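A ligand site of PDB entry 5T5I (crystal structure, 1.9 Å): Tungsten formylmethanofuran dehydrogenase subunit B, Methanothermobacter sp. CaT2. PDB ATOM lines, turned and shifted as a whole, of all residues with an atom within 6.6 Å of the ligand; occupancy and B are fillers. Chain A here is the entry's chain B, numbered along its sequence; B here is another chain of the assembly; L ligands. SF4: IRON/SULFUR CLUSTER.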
ATOM      1  N   CYS A   9       6.658 -27.492   4.020  1.00  0.00           N
ATOM      2  CA  CYS A   9       5.573 -27.116   4.915  1.00  0.00           C
ATOM      3  C   CYS A   9       4.288 -26.803   4.144  1.00  0.00           C
ATOM      4  O   CYS A   9       4.283 -25.844   3.362  1.00  0.00           O
ATOM      5  CB  CYS A   9       5.953 -25.945   5.800  1.00  0.00           C
ATOM      6  SG  CYS A   9       4.635 -25.426   6.938  1.00  0.00           S
ATOM      7  N   PRO A  10       3.163 -27.495   4.428  1.00  0.00           N
ATOM      8  CA  PRO A  10       1.915 -27.171   3.712  1.00  0.00           C
ATOM      9  C   PRO A  10       1.074 -26.128   4.453  1.00  0.00           C
ATOM     10  O   PRO A  10      -0.102 -26.389   4.722  1.00  0.00           O
ATOM     11  CB  PRO A  10       1.213 -28.537   3.642  1.00  0.00           C
ATOM     12  CG  PRO A  10       1.608 -29.195   4.927  1.00  0.00           C
ATOM     13  CD  PRO A  10       2.967 -28.659   5.316  1.00  0.00           C
ATOM     14  N   PHE A  11       1.599 -24.944   4.740  1.00  0.00           N
ATOM     15  CA  PHE A  11       0.755 -23.902   5.363  1.00  0.00           C
ATOM     16  C   PHE A  11       0.765 -22.589   4.569  1.00  0.00           C
ATOM     17  O   PHE A  11      -0.219 -22.335   3.881  1.00  0.00           O
ATOM     18  CB  PHE A  11       1.026 -23.681   6.855  1.00  0.00           C
ATOM     19  CG  PHE A  11       0.042 -22.690   7.451  1.00  0.00           C
ATOM     20  CD1 PHE A  11      -1.269 -23.055   7.712  1.00  0.00           C
ATOM     21  CD2 PHE A  11       0.377 -21.345   7.576  1.00  0.00           C
ATOM     22  CE1 PHE A  11      -2.218 -22.100   8.117  1.00  0.00           C
ATOM     23  CE2 PHE A  11      -0.577 -20.392   7.935  1.00  0.00           C
ATOM     24  CZ  PHE A  11      -1.850 -20.792   8.255  1.00  0.00           C
ATOM     25  N   CYS A  12       1.829 -21.732   4.672  1.00  0.00           N
ATOM     26  CA  CYS A  12       1.783 -20.437   3.964  1.00  0.00           C
ATOM     27  C   CYS A  12       2.639 -20.399   2.698  1.00  0.00           C
ATOM     28  O   CYS A  12       3.369 -21.339   2.405  1.00  0.00           O
ATOM     29  CB  CYS A  12       2.090 -19.262   4.904  1.00  0.00           C
ATOM     30  SG  CYS A  12       3.848 -19.041   5.345  1.00  0.00           S
ATOM     31  N   GLY A  13       2.506 -19.300   1.952  1.00  0.00           N
ATOM     32  CA  GLY A  13       3.214 -19.044   0.692  1.00  0.00           C
ATOM     33  C   GLY A  13       4.727 -18.921   0.781  1.00  0.00           C
ATOM     34  O   GLY A  13       5.379 -18.805  -0.247  1.00  0.00           O
ATOM     35  N   THR A  14       5.311 -18.896   2.002  1.00  0.00           N
ATOM     36  CA  THR A  14       6.771 -18.926   2.197  1.00  0.00           C
ATOM     37  C   THR A  14       7.300 -20.314   1.748  1.00  0.00           C
ATOM     38  O   THR A  14       8.438 -20.402   1.302  1.00  0.00           O
ATOM     39  CB  THR A  14       7.133 -18.567   3.665  1.00  0.00           C
ATOM     40  OG1 THR A  14       6.464 -17.362   4.010  1.00  0.00           O
ATOM     41  CG2 THR A  14       8.623 -18.362   3.879  1.00  0.00           C
ATOM     42  N   LEU A  15       6.470 -21.374   1.867  1.00  0.00           N
ATOM     43  CA  LEU A  15       6.756 -22.724   1.416  1.00  0.00           C
ATOM     44  C   LEU A  15       8.160 -23.227   1.799  1.00  0.00           C
ATOM     45  O   LEU A  15       8.926 -23.682   0.946  1.00  0.00           O
ATOM     46  CB  LEU A  15       6.499 -22.808  -0.112  1.00  0.00           C
ATOM     47  CG  LEU A  15       6.297 -24.228  -0.684  1.00  0.00           C
ATOM     48  CD1 LEU A  15       5.039 -24.880  -0.161  1.00  0.00           C
ATOM     49  CD2 LEU A  15       6.224 -24.198  -2.213  1.00  0.00           C
ATOM     50  N   CYS A  16       8.459 -23.194   3.107  1.00  0.00           N
ATOM     51  CA  CYS A  16       9.719 -23.651   3.683  1.00  0.00           C
ATOM     52  C   CYS A  16       9.931 -25.105   3.314  1.00  0.00           C
ATOM     53  O   CYS A  16       9.011 -25.897   3.468  1.00  0.00           O
ATOM     54  CB  CYS A  16       9.716 -23.474   5.194  1.00  0.00           C
ATOM     55  SG  CYS A  16       9.511 -21.759   5.741  1.00  0.00           S
ATOM     56  N   ASP A  17      11.114 -25.426   2.802  1.00  0.00           N
ATOM     57  CA  ASP A  17      11.457 -26.772   2.344  1.00  0.00           C
ATOM     58  C   ASP A  17      12.653 -27.376   3.097  1.00  0.00           C
ATOM     59  O   ASP A  17      13.313 -28.277   2.598  1.00  0.00           O
ATOM     60  CB  ASP A  17      11.672 -26.769   0.824  1.00  0.00           C
ATOM     61  CG  ASP A  17      12.958 -26.118   0.352  1.00  0.00           C
ATOM     62  OD1 ASP A  17      13.235 -24.969   0.753  1.00  0.00           O
ATOM     63  OD2 ASP A  17      13.720 -26.779  -0.402  1.00  0.00           O
ATOM     64  N   ASP A  18      12.865 -26.922   4.335  1.00  0.00           N
ATOM     65  CA  ASP A  18      13.937 -27.406   5.219  1.00  0.00           C
ATOM     66  C   ASP A  18      13.334 -27.972   6.525  1.00  0.00           C
ATOM     67  O   ASP A  18      14.031 -28.049   7.547  1.00  0.00           O
ATOM     68  CB  ASP A  18      14.893 -26.253   5.559  1.00  0.00           C
ATOM     69  CG  ASP A  18      14.233 -25.097   6.313  1.00  0.00           C
ATOM     70  OD1 ASP A  18      12.980 -25.056   6.366  1.00  0.00           O
ATOM     71  OD2 ASP A  18      14.962 -24.247   6.825  1.00  0.00           O
ATOM     72  N   ILE A  19      12.052 -28.358   6.491  1.00  0.00           N
ATOM     73  CA  ILE A  19      11.397 -28.888   7.683  1.00  0.00           C
ATOM     74  C   ILE A  19      11.920 -30.283   8.017  1.00  0.00           C
ATOM     75  O   ILE A  19      12.183 -31.098   7.111  1.00  0.00           O
ATOM     76  CB  ILE A  19       9.839 -28.888   7.533  1.00  0.00           C
ATOM     77  CG1 ILE A  19       9.274 -27.476   7.153  1.00  0.00           C
ATOM     78  CG2 ILE A  19       9.138 -29.424   8.801  1.00  0.00           C
ATOM     79  CD1 ILE A  19       9.843 -26.278   7.922  1.00  0.00           C
ATOM     80  N   ASN A  33      12.530 -26.784  12.946  1.00  0.00           N
ATOM     81  CA  ASN A  33      12.609 -25.642  12.032  1.00  0.00           C
ATOM     82  C   ASN A  33      11.252 -25.001  11.709  1.00  0.00           C
ATOM     83  O   ASN A  33      11.209 -23.791  11.553  1.00  0.00           O
ATOM     84  CB  ASN A  33      13.378 -25.947  10.729  1.00  0.00           C
ATOM     85  CG  ASN A  33      14.786 -26.410  10.992  1.00  0.00           C
ATOM     86  OD1 ASN A  33      15.440 -25.963  11.943  1.00  0.00           O
ATOM     87  ND2 ASN A  33      15.325 -27.245  10.128  1.00  0.00           N
ATOM     88  N   ALA A  34      10.154 -25.779  11.640  1.00  0.00           N
ATOM     89  CA  ALA A  34       8.833 -25.200  11.344  1.00  0.00           C
ATOM     90  C   ALA A  34       8.443 -24.218  12.450  1.00  0.00           C
ATOM     91  O   ALA A  34       8.726 -24.463  13.628  1.00  0.00           O
ATOM     92  CB  ALA A  34       7.793 -26.297  11.258  1.00  0.00           C
ATOM     93  N   CYS A  35       7.788 -23.128  12.070  1.00  0.00           N
ATOM     94  CA  CYS A  35       7.322 -22.131  13.033  1.00  0.00           C
ATOM     95  C   CYS A  35       6.146 -22.690  13.849  1.00  0.00           C
ATOM     96  O   CYS A  35       5.742 -23.839  13.627  1.00  0.00           O
ATOM     97  CB  CYS A  35       6.925 -20.838  12.305  1.00  0.00           C
ATOM     98  SG  CYS A  35       5.425 -20.977  11.301  1.00  0.00           S
ATOM     99  N   ARG A  36       5.570 -21.888  14.767  1.00  0.00           N
ATOM    100  CA  ARG A  36       4.417 -22.355  15.582  1.00  0.00           C
ATOM    101  C   ARG A  36       3.223 -22.802  14.723  1.00  0.00           C
ATOM    102  O   ARG A  36       2.543 -23.762  15.088  1.00  0.00           O
ATOM    103  CB  ARG A  36       3.976 -21.243  16.553  1.00  0.00           C
ATOM    104  CG  ARG A  36       2.814 -21.649  17.467  1.00  0.00           C
ATOM    105  CD  ARG A  36       2.411 -20.505  18.384  1.00  0.00           C
ATOM    106  NE  ARG A  36       3.380 -20.266  19.453  1.00  0.00           N
ATOM    107  CZ  ARG A  36       3.418 -20.929  20.613  1.00  0.00           C
ATOM    108  NH1 ARG A  36       2.570 -21.918  20.851  1.00  0.00           N
ATOM    109  NH2 ARG A  36       4.318 -20.604  21.532  1.00  0.00           N
ATOM    110  N   ILE A  37       2.980 -22.128  13.590  1.00  0.00           N
ATOM    111  CA  ILE A  37       1.849 -22.480  12.740  1.00  0.00           C
ATOM    112  C   ILE A  37       2.134 -23.780  11.984  1.00  0.00           C
ATOM    113  O   ILE A  37       1.285 -24.670  11.973  1.00  0.00           O
ATOM    114  CB  ILE A  37       1.431 -21.382  11.727  1.00  0.00           C
ATOM    115  CG1 ILE A  37       1.334 -19.979  12.358  1.00  0.00           C
ATOM    116  CG2 ILE A  37       0.076 -21.810  11.105  1.00  0.00           C
ATOM    117  CD1 ILE A  37       1.114 -18.842  11.291  1.00  0.00           C
ATOM    118  N   GLY A  38       3.274 -23.841  11.306  1.00  0.00           N
ATOM    119  CA  GLY A  38       3.653 -25.027  10.540  1.00  0.00           C
ATOM    120  C   GLY A  38       3.630 -26.275  11.394  1.00  0.00           C
ATOM    121  O   GLY A  38       3.031 -27.269  11.016  1.00  0.00           O
ATOM    122  N   HIS A  39       4.203 -26.185  12.603  1.00  0.00           N
ATOM    123  CA  HIS A  39       4.214 -27.282  13.574  1.00  0.00           C
ATOM    124  C   HIS A  39       2.774 -27.720  13.927  1.00  0.00           C
ATOM    125  O   HIS A  39       2.502 -28.906  14.001  1.00  0.00           O
ATOM    126  CB  HIS A  39       4.992 -26.892  14.847  1.00  0.00           C
ATOM    127  CG  HIS A  39       4.889 -27.891  15.935  1.00  0.00           C
ATOM    128  ND1 HIS A  39       5.637 -29.061  15.929  1.00  0.00           N
ATOM    129  CD2 HIS A  39       4.062 -27.907  17.013  1.00  0.00           C
ATOM    130  CE1 HIS A  39       5.277 -29.716  17.028  1.00  0.00           C
ATOM    131  NE2 HIS A  39       4.331 -29.063  17.695  1.00  0.00           N
ATOM    132  N   PHE A  42       1.355 -29.905  11.135  1.00  0.00           N
ATOM    133  CA  PHE A  42       1.975 -31.232  11.126  1.00  0.00           C
ATOM    134  C   PHE A  42       1.505 -32.197  12.237  1.00  0.00           C
ATOM    135  O   PHE A  42       1.317 -33.370  11.945  1.00  0.00           O
ATOM    136  CB  PHE A  42       3.513 -31.123  11.169  1.00  0.00           C
ATOM    137  CG  PHE A  42       4.130 -30.838   9.823  1.00  0.00           C
ATOM    138  CD1 PHE A  42       4.190 -31.825   8.849  1.00  0.00           C
ATOM    139  CD2 PHE A  42       4.681 -29.602   9.533  1.00  0.00           C
ATOM    140  CE1 PHE A  42       4.793 -31.578   7.612  1.00  0.00           C
ATOM    141  CE2 PHE A  42       5.284 -29.355   8.297  1.00  0.00           C
ATOM    142  CZ  PHE A  42       5.313 -30.343   7.344  1.00  0.00           C
ATOM    143  N   ALA A 156       1.795 -13.797  10.141  1.00  0.00           N
ATOM    144  CA  ALA A 156       1.215 -14.469   8.956  1.00  0.00           C
ATOM    145  C   ALA A 156       2.193 -15.257   8.037  1.00  0.00           C
ATOM    146  O   ALA A 156       1.758 -16.159   7.342  1.00  0.00           O
ATOM    147  CB  ALA A 156       0.463 -13.433   8.121  1.00  0.00           C
ATOM    148  N   HIS A 157       3.497 -14.963   8.047  1.00  0.00           N
ATOM    149  CA  HIS A 157       4.483 -15.714   7.236  1.00  0.00           C
ATOM    150  C   HIS A 157       5.684 -15.784   8.173  1.00  0.00           C
ATOM    151  O   HIS A 157       6.636 -15.012   7.974  1.00  0.00           O
ATOM    152  CB  HIS A 157       4.796 -14.958   5.934  1.00  0.00           C
ATOM    153  CG  HIS A 157       3.657 -14.886   4.955  1.00  0.00           C
ATOM    154  ND1 HIS A 157       2.773 -13.818   4.975  1.00  0.00           N
ATOM    155  CD2 HIS A 157       3.362 -15.686   3.909  1.00  0.00           C
ATOM    156  CE1 HIS A 157       1.920 -14.039   3.983  1.00  0.00           C
ATOM    157  NE2 HIS A 157       2.248 -15.138   3.298  1.00  0.00           N
ATOM    158  N   PRO A 158       5.574 -16.526   9.301  1.00  0.00           N
ATOM    159  CA  PRO A 158       6.513 -16.296  10.421  1.00  0.00           C
ATOM    160  C   PRO A 158       7.997 -16.446  10.142  1.00  0.00           C
ATOM    161  O   PRO A 158       8.737 -15.687  10.752  1.00  0.00           O
ATOM    162  CB  PRO A 158       6.035 -17.264  11.499  1.00  0.00           C
ATOM    163  CG  PRO A 158       4.583 -17.385  11.236  1.00  0.00           C
ATOM    164  CD  PRO A 158       4.475 -17.420   9.745  1.00  0.00           C
ATOM    165  N   ARG A 159       8.443 -17.300   9.208  1.00  0.00           N
ATOM    166  CA  ARG A 159       9.886 -17.407   8.915  1.00  0.00           C
ATOM    167  C   ARG A 159      10.339 -16.558   7.746  1.00  0.00           C
ATOM    168  O   ARG A 159      11.506 -16.646   7.352  1.00  0.00           O
ATOM    169  CB  ARG A 159      10.264 -18.884   8.668  1.00  0.00           C
ATOM    170  CG  ARG A 159       9.905 -19.794   9.835  1.00  0.00           C
ATOM    171  CD  ARG A 159      10.276 -21.217   9.510  1.00  0.00           C
ATOM    172  NE  ARG A 159      11.731 -21.397   9.449  1.00  0.00           N
ATOM    173  CZ  ARG A 159      12.359 -22.338   8.754  1.00  0.00           C
ATOM    174  NH1 ARG A 159      11.667 -23.202   8.002  1.00  0.00           N
ATOM    175  NH2 ARG A 159      13.675 -22.428   8.774  1.00  0.00           N
ATOM    176  N   HIS A 160       9.449 -15.704   7.190  1.00  0.00           N
ATOM    177  CA  HIS A 160       9.760 -14.901   6.017  1.00  0.00           C
ATOM    178  C   HIS A 160      10.892 -13.896   6.251  1.00  0.00           C
ATOM    179  O   HIS A 160      11.783 -13.794   5.403  1.00  0.00           O
ATOM    180  CB  HIS A 160       8.473 -14.218   5.517  1.00  0.00           C
ATOM    181  CG  HIS A 160       8.541 -13.672   4.134  1.00  0.00           C
ATOM    182  ND1 HIS A 160       9.127 -12.451   3.867  1.00  0.00           N
ATOM    183  CD2 HIS A 160       8.010 -14.176   2.991  1.00  0.00           C
ATOM    184  CE1 HIS A 160       8.937 -12.251   2.571  1.00  0.00           C
ATOM    185  NE2 HIS A 160       8.301 -13.273   2.003  1.00  0.00           N
ATOM    186  N   ARG A 163      14.395 -15.695   6.779  1.00  0.00           N
ATOM    187  CA  ARG A 163      14.876 -16.235   5.506  1.00  0.00           C
ATOM    188  C   ARG A 163      15.331 -15.168   4.495  1.00  0.00           C
ATOM    189  O   ARG A 163      16.212 -15.440   3.679  1.00  0.00           O
ATOM    190  CB  ARG A 163      13.783 -17.101   4.867  1.00  0.00           C
ATOM    191  CG  ARG A 163      13.609 -18.488   5.523  1.00  0.00           C
ATOM    192  CD  ARG A 163      12.580 -19.343   4.799  1.00  0.00           C
ATOM    193  NE  ARG A 163      12.991 -19.563   3.415  1.00  0.00           N
ATOM    194  CZ  ARG A 163      12.251 -20.104   2.449  1.00  0.00           C
ATOM    195  NH1 ARG A 163      11.027 -20.524   2.706  1.00  0.00           N
ATOM    196  NH2 ARG A 163      12.737 -20.225   1.225  1.00  0.00           N
ATOM    197  N   TYR A 291      -0.029 -22.040   0.998  1.00  0.00           N
ATOM    198  CA  TYR A 291       1.136 -22.699   0.381  1.00  0.00           C
ATOM    199  C   TYR A 291       0.922 -23.044  -1.113  1.00  0.00           C
ATOM    200  O   TYR A 291       1.902 -23.123  -1.843  1.00  0.00           O
ATOM    201  CB  TYR A 291       1.562 -23.936   1.186  1.00  0.00           C
ATOM    202  CG  TYR A 291       0.721 -25.170   0.922  1.00  0.00           C
ATOM    203  CD1 TYR A 291      -0.449 -25.407   1.642  1.00  0.00           C
ATOM    204  CD2 TYR A 291       1.132 -26.128   0.000  1.00  0.00           C
ATOM    205  CE1 TYR A 291      -1.205 -26.542   1.415  1.00  0.00           C
ATOM    206  CE2 TYR A 291       0.381 -27.274  -0.234  1.00  0.00           C
ATOM    207  CZ  TYR A 291      -0.790 -27.482   0.481  1.00  0.00           C
ATOM    208  OH  TYR A 291      -1.546 -28.601   0.255  1.00  0.00           O
ATOM    209  N   GLY B  14       8.234 -18.965  16.855  1.00  0.00           N
ATOM    210  CA  GLY B  14       9.043 -19.906  16.099  1.00  0.00           C
ATOM    211  C   GLY B  14       9.498 -19.299  14.786  1.00  0.00           C
ATOM    212  O   GLY B  14       9.715 -20.026  13.816  1.00  0.00           O
HETATM  213 FE1  SF4 L   1       7.433 -21.703   6.720  1.00  0.00          FE
HETATM  214 FE2  SF4 L   1       4.891 -20.668   6.496  1.00  0.00          FE
HETATM  215 FE3  SF4 L   1       5.993 -21.324   9.076  1.00  0.00          FE
HETATM  216 FE4  SF4 L   1       5.288 -23.329   7.281  1.00  0.00          FE
HETATM  217  S1  SF4 L   1       3.979 -21.758   8.139  1.00  0.00           S
HETATM  218  S2  SF4 L   1       7.171 -23.084   8.498  1.00  0.00           S
HETATM  219  S3  SF4 L   1       5.772 -22.290   5.226  1.00  0.00           S
HETATM  220  S4  SF4 L   1       6.691 -19.757   7.568  1.00  0.00           S
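An iron atom (FE4) of the ligand is bound by the side-chain sulfur of Cys 9.
The side-chain sulfur of Cys 12 is bound to an iron atom (FE2) of the ligand.
N of Cys 16 lies close to S3 of the ligand (3.5 Å).
SG of Cys 16 is bound to FE1 of the ligand (2.3 Å).
N of Cys 35 lies close to S2 of the ligand (3.6 Å).
SG of Cys 35 is bound to FE3 of the ligand, at 2.3 Å.
N of Arg 159 sits close to S4 of the ligand (3.4 Å).
The backbone NH of Leu 15 lies close to a sulfur (S3) of the ligand (3.6 Å).
N of Cys 9 is in hydrogen-bond range of O of Cys 16 (2.9 Å).
The side-chain sulfur of Cys 9 lies close to the backbone NH of Phe 11, at 3.8 Å.
SG of Cys 16 lies close to NH1 of Arg 159.
The side-chain sulfur of Cys 16 lies close to the guanidinium group of Arg 163 (3.6 Å).
The side-chain sulfur of Cys 35 lies close to the backbone NH of Gly 38 (3.6 Å).
SG of Cys 35 sits close to N of Ile 37, 3.5 Å away.
The backbone carbonyl oxygen (O) of Asn 33 lies within hydrogen-bond range of the guanidinium group (NE) of Arg 159 (3.2 Å).
The backbone carbonyl oxygen (O) of Phe 11 sits at hydrogen-bond distance from the backbone NH (N) of Tyr 291 (2.9 Å).
Residues that only touch the ligand: Phe 11 (3.7 Å), Pro 158 (3.8 Å), Gly 38 (3.9 Å) and Ala 34 (3.9 Å).
Hydrophobic or aromatic side chains within 4 Å of the ligand: Phe 11 and Pro 158.
Ten residues have an atom within 4 Å of the ligand: Cys 9, Phe 11, Cys 12, Leu 15, Cys 16, Ala 34, Cys 35, Gly 38, Pro 158 and Arg 159.
The nearest printed residue that does not touch the ligand is Thr 14 of chain A (4.1 Å).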
